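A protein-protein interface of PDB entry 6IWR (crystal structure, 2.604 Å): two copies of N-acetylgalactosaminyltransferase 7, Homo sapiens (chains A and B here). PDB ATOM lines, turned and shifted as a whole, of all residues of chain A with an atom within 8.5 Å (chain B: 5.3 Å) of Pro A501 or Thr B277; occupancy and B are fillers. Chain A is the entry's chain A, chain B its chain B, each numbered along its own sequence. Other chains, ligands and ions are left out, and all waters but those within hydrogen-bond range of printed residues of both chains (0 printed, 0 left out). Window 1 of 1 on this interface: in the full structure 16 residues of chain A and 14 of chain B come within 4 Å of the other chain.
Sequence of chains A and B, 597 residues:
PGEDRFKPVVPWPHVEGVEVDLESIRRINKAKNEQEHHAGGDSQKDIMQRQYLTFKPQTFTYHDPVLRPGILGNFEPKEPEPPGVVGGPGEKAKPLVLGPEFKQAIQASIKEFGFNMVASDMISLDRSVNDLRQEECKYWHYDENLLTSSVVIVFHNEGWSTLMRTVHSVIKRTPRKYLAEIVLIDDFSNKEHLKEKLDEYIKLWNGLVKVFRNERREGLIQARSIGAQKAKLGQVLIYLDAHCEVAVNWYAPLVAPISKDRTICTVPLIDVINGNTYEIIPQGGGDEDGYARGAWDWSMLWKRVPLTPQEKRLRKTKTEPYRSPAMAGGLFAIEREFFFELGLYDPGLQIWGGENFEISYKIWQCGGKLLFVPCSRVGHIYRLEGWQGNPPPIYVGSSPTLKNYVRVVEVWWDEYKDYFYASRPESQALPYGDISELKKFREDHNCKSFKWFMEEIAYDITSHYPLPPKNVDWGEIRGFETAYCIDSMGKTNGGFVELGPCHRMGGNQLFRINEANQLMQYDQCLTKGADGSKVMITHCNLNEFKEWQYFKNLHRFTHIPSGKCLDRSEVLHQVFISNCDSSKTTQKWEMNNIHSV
The backbone NH (N) of Cys A502 is in hydrogen-bond range of the backbone carbonyl oxygen (O) of Ala A483 (2.9 Å).
NE2 of Gln A509 is in hydrogen-bond range of O of Pro A501 (2.8 Å).
The backbone NH (N) of Met A505 sits at hydrogen-bond distance from a ring nitrogen (ND1) of His A503 (2.9 Å).
The backbone NH (N) of His A503 lies within hydrogen-bond range of the side-chain amide oxygen (OE1) of Gln A509, at 3.1 Å.
N of Leu B96 is in hydrogen-bond range of O of Thr B277, 3.0 Å away.
N of Asn B274 sits at hydrogen-bond distance from O of Glu B279, 3.1 Å away.
A ring nitrogen (NE2) of His A573 is in hydrogen-bond range of the side-chain carboxylate (OE2) of Glu B279 (2.8 Å).
Of the 11 printed residues of chain B, 4 touch a printed residue of chain A.
Among the printed residues, no Asp or Glu carboxylate lies within 4 Å of a Lys or Arg side-chain nitrogen of the other chain.
No position is printed for both chains.
CB of Pro B95 touches CB of Pro A501, 3.8 Å away.
Val B97 touches Pro A501.
CG of Pro A501 touches OG1 of Thr B277, 3.6 Å away.
Pro A501 touches Glu B279.
Cys A502 touches Val B97.
CG1 of Val B97 touches CB of His A503 (3.9 Å).
Pro A501 touches just these residues of chain B: Pro B95, Val B97, Thr B277 and Glu B279.
Thr B277 touches just one residue of chain A: Pro A501 (3.6 Å).
No residue of chain A comes within 4 Å of Asn B276.
Of the printed residues of chain B, Cys A502 touches Val B97.
Printed residues of chain A within 4 Å of Pro B95: Pro A501 (3.8 Å).
Of the printed residues of chain B, His A573 touches Glu B279 (2.8 Å).
The nearest residue of chain B that does not touch Pro A501 is Asn B274 (4.8 Å).
The nearest residue of chain A that does not touch Thr B277 is His A573 (6.4 Å).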
ATOM      1  N   GLU A 476     -25.723 -24.794  -5.532  1.00  0.00           N
ATOM      2  CA  GLU A 476     -25.215 -23.721  -6.372  1.00  0.00           C
ATOM      3  C   GLU A 476     -23.774 -23.396  -5.976  1.00  0.00           C
ATOM      4  O   GLU A 476     -23.365 -23.571  -4.820  1.00  0.00           O
ATOM      5  CB  GLU A 476     -26.087 -22.474  -6.223  1.00  0.00           C
ATOM      6  CG  GLU A 476     -25.945 -21.789  -4.862  1.00  0.00           C
ATOM      7  CD  GLU A 476     -26.804 -20.548  -4.701  1.00  0.00           C
ATOM      8  OE1 GLU A 476     -26.635 -19.848  -3.679  1.00  0.00           O
ATOM      9  OE2 GLU A 476     -27.631 -20.247  -5.582  1.00  0.00           O
ATOM     10  N   ARG A 478     -22.034 -20.119  -5.872  1.00  0.00           N
ATOM     11  CA  ARG A 478     -22.391 -18.715  -5.953  1.00  0.00           C
ATOM     12  C   ARG A 478     -21.188 -17.855  -5.608  1.00  0.00           C
ATOM     13  O   ARG A 478     -20.384 -18.208  -4.748  1.00  0.00           O
ATOM     14  CB  ARG A 478     -23.554 -18.412  -5.006  1.00  0.00           C
ATOM     15  CG  ARG A 478     -23.921 -16.948  -4.904  1.00  0.00           C
ATOM     16  CD  ARG A 478     -24.883 -16.750  -3.760  1.00  0.00           C
ATOM     17  NE  ARG A 478     -26.193 -17.280  -4.109  1.00  0.00           N
ATOM     18  CZ  ARG A 478     -27.220 -16.555  -4.551  1.00  0.00           C
ATOM     19  NH1 ARG A 478     -28.373 -17.150  -4.852  1.00  0.00           N
ATOM     20  NH2 ARG A 478     -27.093 -15.248  -4.709  1.00  0.00           N
ATOM     21  N   THR A 482     -22.365 -12.061  -3.914  1.00  0.00           N
ATOM     22  CA  THR A 482     -22.836 -11.668  -5.235  1.00  0.00           C
ATOM     23  C   THR A 482     -24.094 -12.460  -5.565  1.00  0.00           C
ATOM     24  O   THR A 482     -24.524 -13.357  -4.832  1.00  0.00           O
ATOM     25  CB  THR A 482     -21.816 -11.927  -6.358  1.00  0.00           C
ATOM     26  OG1 THR A 482     -22.020 -13.253  -6.881  1.00  0.00           O
ATOM     27  CG2 THR A 482     -20.371 -11.769  -5.890  1.00  0.00           C
ATOM     28  N   ALA A 483     -24.663 -12.137  -6.709  1.00  0.00           N
ATOM     29  CA  ALA A 483     -25.835 -12.819  -7.224  1.00  0.00           C
ATOM     30  C   ALA A 483     -25.491 -13.563  -8.510  1.00  0.00           C
ATOM     31  O   ALA A 483     -26.348 -13.774  -9.367  1.00  0.00           O
ATOM     32  CB  ALA A 483     -26.960 -11.817  -7.446  1.00  0.00           C
ATOM     33  N   TYR A 484     -24.224 -13.933  -8.671  1.00  0.00           N
ATOM     34  CA  TYR A 484     -23.772 -14.667  -9.836  1.00  0.00           C
ATOM     35  C   TYR A 484     -23.384 -16.075  -9.434  1.00  0.00           C
ATOM     36  O   TYR A 484     -22.823 -16.290  -8.358  1.00  0.00           O
ATOM     37  CB  TYR A 484     -22.607 -13.963 -10.505  1.00  0.00           C
ATOM     38  CG  TYR A 484     -22.999 -12.656 -11.141  1.00  0.00           C
ATOM     39  CD1 TYR A 484     -23.802 -12.626 -12.294  1.00  0.00           C
ATOM     40  CD2 TYR A 484     -22.557 -11.445 -10.614  1.00  0.00           C
ATOM     41  CE1 TYR A 484     -24.159 -11.406 -12.911  1.00  0.00           C
ATOM     42  CE2 TYR A 484     -22.908 -10.225 -11.218  1.00  0.00           C
ATOM     43  CZ  TYR A 484     -23.714 -10.213 -12.360  1.00  0.00           C
ATOM     44  OH  TYR A 484     -24.056  -9.012 -12.946  1.00  0.00           O
ATOM     45  N   CYS A 485     -23.727 -17.028 -10.291  1.00  0.00           N
ATOM     46  CA  CYS A 485     -23.551 -18.451 -10.055  1.00  0.00           C
ATOM     47  C   CYS A 485     -22.817 -19.066 -11.243  1.00  0.00           C
ATOM     48  O   CYS A 485     -22.994 -18.645 -12.392  1.00  0.00           O
ATOM     49  CB  CYS A 485     -24.904 -19.166  -9.869  1.00  0.00           C
ATOM     50  SG  CYS A 485     -25.597 -19.066  -8.200  1.00  0.00           S
ATOM     51  N   ILE A 486     -21.970 -20.056 -10.962  1.00  0.00           N
ATOM     52  CA  ILE A 486     -21.447 -20.847 -12.057  1.00  0.00           C
ATOM     53  C   ILE A 486     -22.622 -21.599 -12.634  1.00  0.00           C
ATOM     54  O   ILE A 486     -23.513 -22.048 -11.899  1.00  0.00           O
ATOM     55  CB  ILE A 486     -20.319 -21.789 -11.604  1.00  0.00           C
ATOM     56  CG1 ILE A 486     -19.159 -20.970 -10.991  1.00  0.00           C
ATOM     57  CG2 ILE A 486     -19.850 -22.632 -12.789  1.00  0.00           C
ATOM     58  CD1 ILE A 486     -17.934 -21.762 -10.551  1.00  0.00           C
ATOM     59  N   ASP A 487     -22.684 -21.678 -13.960  1.00  0.00           N
ATOM     60  CA  ASP A 487     -23.774 -22.453 -14.509  1.00  0.00           C
ATOM     61  C   ASP A 487     -23.408 -23.004 -15.875  1.00  0.00           C
ATOM     62  O   ASP A 487     -22.624 -22.425 -16.636  1.00  0.00           O
ATOM     63  CB  ASP A 487     -25.071 -21.630 -14.444  1.00  0.00           C
ATOM     64  CG  ASP A 487     -25.741 -21.391 -15.773  1.00  0.00           C
ATOM     65  OD1 ASP A 487     -26.207 -22.324 -16.466  1.00  0.00           O
ATOM     66  OD2 ASP A 487     -25.893 -20.203 -16.051  1.00  0.00           O
ATOM     67  N   MET A 489     -24.898 -23.788 -18.628  1.00  0.00           N
ATOM     68  CA  MET A 489     -25.613 -23.588 -19.887  1.00  0.00           C
ATOM     69  C   MET A 489     -26.041 -24.919 -20.492  1.00  0.00           C
ATOM     70  O   MET A 489     -26.234 -25.023 -21.702  1.00  0.00           O
ATOM     71  CB  MET A 489     -24.770 -22.807 -20.899  1.00  0.00           C
ATOM     72  CG  MET A 489     -24.236 -21.503 -20.381  1.00  0.00           C
ATOM     73  SD  MET A 489     -25.530 -20.586 -19.569  1.00  0.00           S
ATOM     74  CE  MET A 489     -24.626 -19.074 -19.251  1.00  0.00           C
ATOM     75  N   GLU A 498     -19.878 -21.227 -17.674  1.00  0.00           N
ATOM     76  CA  GLU A 498     -19.909 -19.768 -17.620  1.00  0.00           C
ATOM     77  C   GLU A 498     -20.488 -19.289 -16.296  1.00  0.00           C
ATOM     78  O   GLU A 498     -20.871 -20.076 -15.418  1.00  0.00           O
ATOM     79  CB  GLU A 498     -20.723 -19.200 -18.781  1.00  0.00           C
ATOM     80  CG  GLU A 498     -20.549 -19.983 -20.061  1.00  0.00           C
ATOM     81  CD  GLU A 498     -21.388 -19.438 -21.201  1.00  0.00           C
ATOM     82  OE1 GLU A 498     -21.955 -18.337 -21.038  1.00  0.00           O
ATOM     83  OE2 GLU A 498     -21.481 -20.113 -22.255  1.00  0.00           O
ATOM     84  N   LEU A 499     -20.549 -17.968 -16.165  1.00  0.00           N
ATOM     85  CA  LEU A 499     -21.179 -17.315 -15.028  1.00  0.00           C
ATOM     86  C   LEU A 499     -22.535 -16.775 -15.460  1.00  0.00           C
ATOM     87  O   LEU A 499     -22.673 -16.221 -16.551  1.00  0.00           O
ATOM     88  CB  LEU A 499     -20.304 -16.178 -14.495  1.00  0.00           C
ATOM     89  CG  LEU A 499     -20.577 -15.657 -13.080  1.00  0.00           C
ATOM     90  CD1 LEU A 499     -20.007 -16.634 -12.084  1.00  0.00           C
ATOM     91  CD2 LEU A 499     -20.017 -14.241 -12.857  1.00  0.00           C
ATOM     92  N   GLY A 500     -23.543 -16.947 -14.616  1.00  0.00           N
ATOM     93  CA  GLY A 500     -24.824 -16.338 -14.887  1.00  0.00           C
ATOM     94  C   GLY A 500     -25.505 -15.895 -13.614  1.00  0.00           C
ATOM     95  O   GLY A 500     -25.075 -16.228 -12.508  1.00  0.00           O
ATOM     96  N   PRO A 501     -26.583 -15.128 -13.745  1.00  0.00           N
ATOM     97  CA  PRO A 501     -27.324 -14.707 -12.553  1.00  0.00           C
ATOM     98  C   PRO A 501     -27.940 -15.910 -11.854  1.00  0.00           C
ATOM     99  O   PRO A 501     -28.507 -16.797 -12.495  1.00  0.00           O
ATOM    100  CB  PRO A 501     -28.390 -13.749 -13.105  1.00  0.00           C
ATOM    101  CG  PRO A 501     -28.303 -13.820 -14.570  1.00  0.00           C
ATOM    102  CD  PRO A 501     -27.022 -14.440 -14.966  1.00  0.00           C
ATOM    103  N   CYS A 502     -27.785 -15.948 -10.532  1.00  0.00           N
ATOM    104  CA  CYS A 502     -28.336 -17.030  -9.726  1.00  0.00           C
ATOM    105  C   CYS A 502     -29.853 -17.001  -9.781  1.00  0.00           C
ATOM    106  O   CYS A 502     -30.475 -15.933  -9.745  1.00  0.00           O
ATOM    107  CB  CYS A 502     -27.883 -16.910  -8.273  1.00  0.00           C
ATOM    108  SG  CYS A 502     -26.093 -17.075  -7.993  1.00  0.00           S
ATOM    109  N   HIS A 503     -30.447 -18.185  -9.863  1.00  0.00           N
ATOM    110  CA  HIS A 503     -31.892 -18.317  -9.778  1.00  0.00           C
ATOM    111  C   HIS A 503     -32.331 -19.366  -8.757  1.00  0.00           C
ATOM    112  O   HIS A 503     -33.540 -19.542  -8.555  1.00  0.00           O
ATOM    113  CB  HIS A 503     -32.473 -18.660 -11.157  1.00  0.00           C
ATOM    114  CG  HIS A 503     -31.844 -19.863 -11.780  1.00  0.00           C
ATOM    115  ND1 HIS A 503     -31.679 -21.054 -11.099  1.00  0.00           N
ATOM    116  CD2 HIS A 503     -31.317 -20.058 -13.009  1.00  0.00           C
ATOM    117  CE1 HIS A 503     -31.085 -21.933 -11.887  1.00  0.00           C
ATOM    118  NE2 HIS A 503     -30.865 -21.357 -13.054  1.00  0.00           N
ATOM    119  N   ARG A 504     -31.399 -20.077  -8.120  1.00  0.00           N
ATOM    120  CA  ARG A 504     -31.736 -20.998  -7.036  1.00  0.00           C
ATOM    121  C   ARG A 504     -32.718 -22.060  -7.479  1.00  0.00           C
ATOM    122  O   ARG A 504     -33.492 -22.555  -6.669  1.00  0.00           O
ATOM    123  CB  ARG A 504     -32.315 -20.271  -5.814  1.00  0.00           C
ATOM    124  CG  ARG A 504     -31.292 -19.522  -4.983  1.00  0.00           C
ATOM    125  CD  ARG A 504     -31.868 -18.988  -3.697  1.00  0.00           C
ATOM    126  NE  ARG A 504     -30.918 -18.065  -3.113  1.00  0.00           N
ATOM    127  CZ  ARG A 504     -31.228 -17.025  -2.334  1.00  0.00           C
ATOM    128  NH1 ARG A 504     -32.499 -16.779  -2.035  1.00  0.00           N
ATOM    129  NH2 ARG A 504     -30.265 -16.226  -1.846  1.00  0.00           N
ATOM    130  N   MET A 505     -32.738 -22.400  -8.763  1.00  0.00           N
ATOM    131  CA  MET A 505     -33.637 -23.432  -9.252  1.00  0.00           C
ATOM    132  C   MET A 505     -32.915 -24.735  -9.548  1.00  0.00           C
ATOM    133  O   MET A 505     -33.521 -25.655 -10.095  1.00  0.00           O
ATOM    134  CB  MET A 505     -34.377 -22.931 -10.481  1.00  0.00           C
ATOM    135  CG  MET A 505     -35.348 -21.801 -10.145  1.00  0.00           C
ATOM    136  SD  MET A 505     -36.567 -22.301  -8.911  1.00  0.00           S
ATOM    137  CE  MET A 505     -37.278 -23.705  -9.753  1.00  0.00           C
ATOM    138  N   GLN A 509     -27.388 -24.860 -12.681  1.00  0.00           N
ATOM    139  CA  GLN A 509     -26.640 -24.093 -11.697  1.00  0.00           C
ATOM    140  C   GLN A 509     -26.369 -24.896 -10.437  1.00  0.00           C
ATOM    141  O   GLN A 509     -26.099 -24.311  -9.380  1.00  0.00           O
ATOM    142  CB  GLN A 509     -27.375 -22.807 -11.355  1.00  0.00           C
ATOM    143  CG  GLN A 509     -27.317 -21.794 -12.443  1.00  0.00           C
ATOM    144  CD  GLN A 509     -27.922 -20.478 -12.025  1.00  0.00           C
ATOM    145  OE1 GLN A 509     -28.414 -20.334 -10.896  1.00  0.00           O
ATOM    146  NE2 GLN A 509     -27.871 -19.497 -12.918  1.00  0.00           N
ATOM    147  N   GLU A 570     -17.490 -11.694 -13.753  1.00  0.00           N
ATOM    148  CA  GLU A 570     -18.745 -10.988 -13.480  1.00  0.00           C
ATOM    149  C   GLU A 570     -19.206 -10.065 -14.585  1.00  0.00           C
ATOM    150  O   GLU A 570     -20.286 -10.228 -15.116  1.00  0.00           O
ATOM    151  CB  GLU A 570     -18.667 -10.166 -12.193  1.00  0.00           C
ATOM    152  CG  GLU A 570     -17.970 -10.835 -11.027  1.00  0.00           C
ATOM    153  CD  GLU A 570     -18.654 -10.567  -9.705  1.00  0.00           C
ATOM    154  OE1 GLU A 570     -19.740  -9.969  -9.721  1.00  0.00           O
ATOM    155  OE2 GLU A 570     -18.119 -10.956  -8.656  1.00  0.00           O
ATOM    156  N   HIS A 573     -19.088 -12.361 -17.412  1.00  0.00           N
ATOM    157  CA  HIS A 573     -19.769 -13.655 -17.216  1.00  0.00           C
ATOM    158  C   HIS A 573     -18.885 -14.860 -17.540  1.00  0.00           C
ATOM    159  O   HIS A 573     -19.264 -15.773 -18.247  1.00  0.00           O
ATOM    160  CB  HIS A 573     -21.071 -13.727 -17.996  1.00  0.00           C
ATOM    161  CG  HIS A 573     -22.150 -12.831 -17.478  1.00  0.00           C
ATOM    162  ND1 HIS A 573     -21.899 -11.743 -16.677  1.00  0.00           N
ATOM    163  CD2 HIS A 573     -23.486 -12.854 -17.667  1.00  0.00           C
ATOM    164  CE1 HIS A 573     -23.033 -11.139 -16.391  1.00  0.00           C
ATOM    165  NE2 HIS A 573     -24.011 -11.798 -16.975  1.00  0.00           N
ATOM    166  N   LYS B  94     -29.327  -4.298 -14.404  1.00  0.00           N
ATOM    167  CA  LYS B  94     -29.240  -5.373 -13.443  1.00  0.00           C
ATOM    168  C   LYS B  94     -30.052  -6.546 -13.919  1.00  0.00           C
ATOM    169  O   LYS B  94     -31.114  -6.356 -14.466  1.00  0.00           O
ATOM    170  CB  LYS B  94     -29.808  -4.892 -12.122  1.00  0.00           C
ATOM    171  CG  LYS B  94     -29.013  -5.309 -10.912  1.00  0.00           C
ATOM    172  CD  LYS B  94     -29.844  -6.161  -9.974  1.00  0.00           C
ATOM    173  CE  LYS B  94     -30.950  -5.367  -9.316  1.00  0.00           C
ATOM    174  NZ  LYS B  94     -31.379  -6.012  -8.051  1.00  0.00           N
ATOM    175  N   PRO B  95     -29.572  -7.760 -13.705  1.00  0.00           N
ATOM    176  CA  PRO B  95     -30.339  -8.922 -14.182  1.00  0.00           C
ATOM    177  C   PRO B  95     -31.683  -8.995 -13.481  1.00  0.00           C
ATOM    178  O   PRO B  95     -31.782  -8.766 -12.276  1.00  0.00           O
ATOM    179  CB  PRO B  95     -29.448 -10.126 -13.847  1.00  0.00           C
ATOM    180  CG  PRO B  95     -28.341  -9.608 -13.045  1.00  0.00           C
ATOM    181  CD  PRO B  95     -28.213  -8.143 -13.287  1.00  0.00           C
ATOM    182  N   LEU B  96     -32.726  -9.271 -14.266  1.00  0.00           N
ATOM    183  CA  LEU B  96     -34.090  -9.469 -13.778  1.00  0.00           C
ATOM    184  C   LEU B  96     -34.382 -10.966 -13.766  1.00  0.00           C
ATOM    185  O   LEU B  96     -34.742 -11.542 -14.793  1.00  0.00           O
ATOM    186  CB  LEU B  96     -35.083  -8.745 -14.667  1.00  0.00           C
ATOM    187  CG  LEU B  96     -36.440  -8.268 -14.151  1.00  0.00           C
ATOM    188  CD1 LEU B  96     -37.469  -8.226 -15.291  1.00  0.00           C
ATOM    189  CD2 LEU B  96     -36.941  -9.074 -12.991  1.00  0.00           C
ATOM    190  N   VAL B  97     -34.218 -11.584 -12.605  1.00  0.00           N
ATOM    191  CA  VAL B  97     -34.499 -12.999 -12.386  1.00  0.00           C
ATOM    192  C   VAL B  97     -35.946 -13.123 -11.902  1.00  0.00           C
ATOM    193  O   VAL B  97     -36.340 -12.443 -10.951  1.00  0.00           O
ATOM    194  CB  VAL B  97     -33.507 -13.593 -11.364  1.00  0.00           C
ATOM    195  CG1 VAL B  97     -33.861 -15.058 -10.996  1.00  0.00           C
ATOM    196  CG2 VAL B  97     -32.058 -13.458 -11.857  1.00  0.00           C
ATOM    197  N   ILE B 123     -39.615  -4.384 -17.870  1.00  0.00           N
ATOM    198  CA  ILE B 123     -38.488  -3.468 -17.891  1.00  0.00           C
ATOM    199  C   ILE B 123     -38.913  -2.228 -18.649  1.00  0.00           C
ATOM    200  O   ILE B 123     -39.601  -2.317 -19.673  1.00  0.00           O
ATOM    201  CB  ILE B 123     -37.249  -4.117 -18.520  1.00  0.00           C
ATOM    202  CG1 ILE B 123     -36.823  -5.316 -17.665  1.00  0.00           C
ATOM    203  CG2 ILE B 123     -36.142  -3.084 -18.671  1.00  0.00           C
ATOM    204  CD1 ILE B 123     -35.782  -6.208 -18.329  1.00  0.00           C
ATOM    205  N   ASN B 274     -28.755 -10.361 -22.609  1.00  0.00           N
ATOM    206  CA  ASN B 274     -29.221 -11.688 -22.251  1.00  0.00           C
ATOM    207  C   ASN B 274     -30.721 -11.765 -22.444  1.00  0.00           C
ATOM    208  O   ASN B 274     -31.479 -11.043 -21.787  1.00  0.00           O
ATOM    209  CB  ASN B 274     -28.846 -11.978 -20.801  1.00  0.00           C
ATOM    210  CG  ASN B 274     -29.262 -13.372 -20.337  1.00  0.00           C
ATOM    211  OD1 ASN B 274     -30.353 -13.877 -20.663  1.00  0.00           O
ATOM    212  ND2 ASN B 274     -28.396 -13.991 -19.539  1.00  0.00           N
ATOM    213  N   GLY B 275     -31.156 -12.642 -23.342  1.00  0.00           N
ATOM    214  CA  GLY B 275     -32.564 -12.712 -23.659  1.00  0.00           C
ATOM    215  C   GLY B 275     -33.449 -13.256 -22.559  1.00  0.00           C
ATOM    216  O   GLY B 275     -34.676 -13.249 -22.702  1.00  0.00           O
ATOM    217  N   ASN B 276     -32.874 -13.763 -21.477  1.00  0.00           N
ATOM    218  CA  ASN B 276     -33.690 -14.140 -20.338  1.00  0.00           C
ATOM    219  C   ASN B 276     -33.767 -13.038 -19.294  1.00  0.00           C
ATOM    220  O   ASN B 276     -34.864 -12.625 -18.927  1.00  0.00           O
ATOM    221  CB  ASN B 276     -33.169 -15.423 -19.699  1.00  0.00           C
ATOM    222  CG  ASN B 276     -34.083 -15.921 -18.612  1.00  0.00           C
ATOM    223  OD1 ASN B 276     -35.311 -15.760 -18.699  1.00  0.00           O
ATOM    224  ND2 ASN B 276     -33.500 -16.475 -17.548  1.00  0.00           N
ATOM    225  N   THR B 277     -32.623 -12.530 -18.831  1.00  0.00           N
ATOM    226  CA  THR B 277     -32.577 -11.615 -17.698  1.00  0.00           C
ATOM    227  C   THR B 277     -32.139 -10.194 -18.048  1.00  0.00           C
ATOM    228  O   THR B 277     -32.335  -9.285 -17.233  1.00  0.00           O
ATOM    229  CB  THR B 277     -31.651 -12.181 -16.611  1.00  0.00           C
ATOM    230  OG1 THR B 277     -30.395 -12.561 -17.193  1.00  0.00           O
ATOM    231  CG2 THR B 277     -32.290 -13.405 -15.979  1.00  0.00           C
ATOM    232  N   TYR B 278     -31.555  -9.976 -19.219  1.00  0.00           N
ATOM    233  CA  TYR B 278     -31.450  -8.666 -19.857  1.00  0.00           C
ATOM    234  C   TYR B 278     -30.254  -7.852 -19.371  1.00  0.00           C
ATOM    235  O   TYR B 278     -30.105  -6.684 -19.776  1.00  0.00           O
ATOM    236  CB  TYR B 278     -32.770  -7.891 -19.714  1.00  0.00           C
ATOM    237  CG  TYR B 278     -33.779  -8.443 -20.680  1.00  0.00           C
ATOM    238  CD1 TYR B 278     -33.862  -7.952 -21.977  1.00  0.00           C
ATOM    239  CD2 TYR B 278     -34.593  -9.523 -20.324  1.00  0.00           C
ATOM    240  CE1 TYR B 278     -34.767  -8.490 -22.879  1.00  0.00           C
ATOM    241  CE2 TYR B 278     -35.487 -10.057 -21.195  1.00  0.00           C
ATOM    242  CZ  TYR B 278     -35.574  -9.553 -22.475  1.00  0.00           C
ATOM    243  OH  TYR B 278     -36.467 -10.114 -23.364  1.00  0.00           O
ATOM    244  N   GLU B 279     -29.387  -8.428 -18.537  1.00  0.00           N
ATOM    245  CA  GLU B 279     -28.116  -7.786 -18.270  1.00  0.00           C
ATOM    246  C   GLU B 279     -27.253  -7.855 -19.527  1.00  0.00           C
ATOM    247  O   GLU B 279     -27.418  -8.743 -20.369  1.00  0.00           O
ATOM    248  CB  GLU B 279     -27.426  -8.431 -17.073  1.00  0.00           C
ATOM    249  CG  GLU B 279     -26.555  -9.639 -17.383  1.00  0.00           C
ATOM    250  CD  GLU B 279     -27.343 -10.945 -17.623  1.00  0.00           C
ATOM    251  OE1 GLU B 279     -28.613 -10.932 -17.564  1.00  0.00           O
ATOM    252  OE2 GLU B 279     -26.676 -11.986 -17.877  1.00  0.00           O
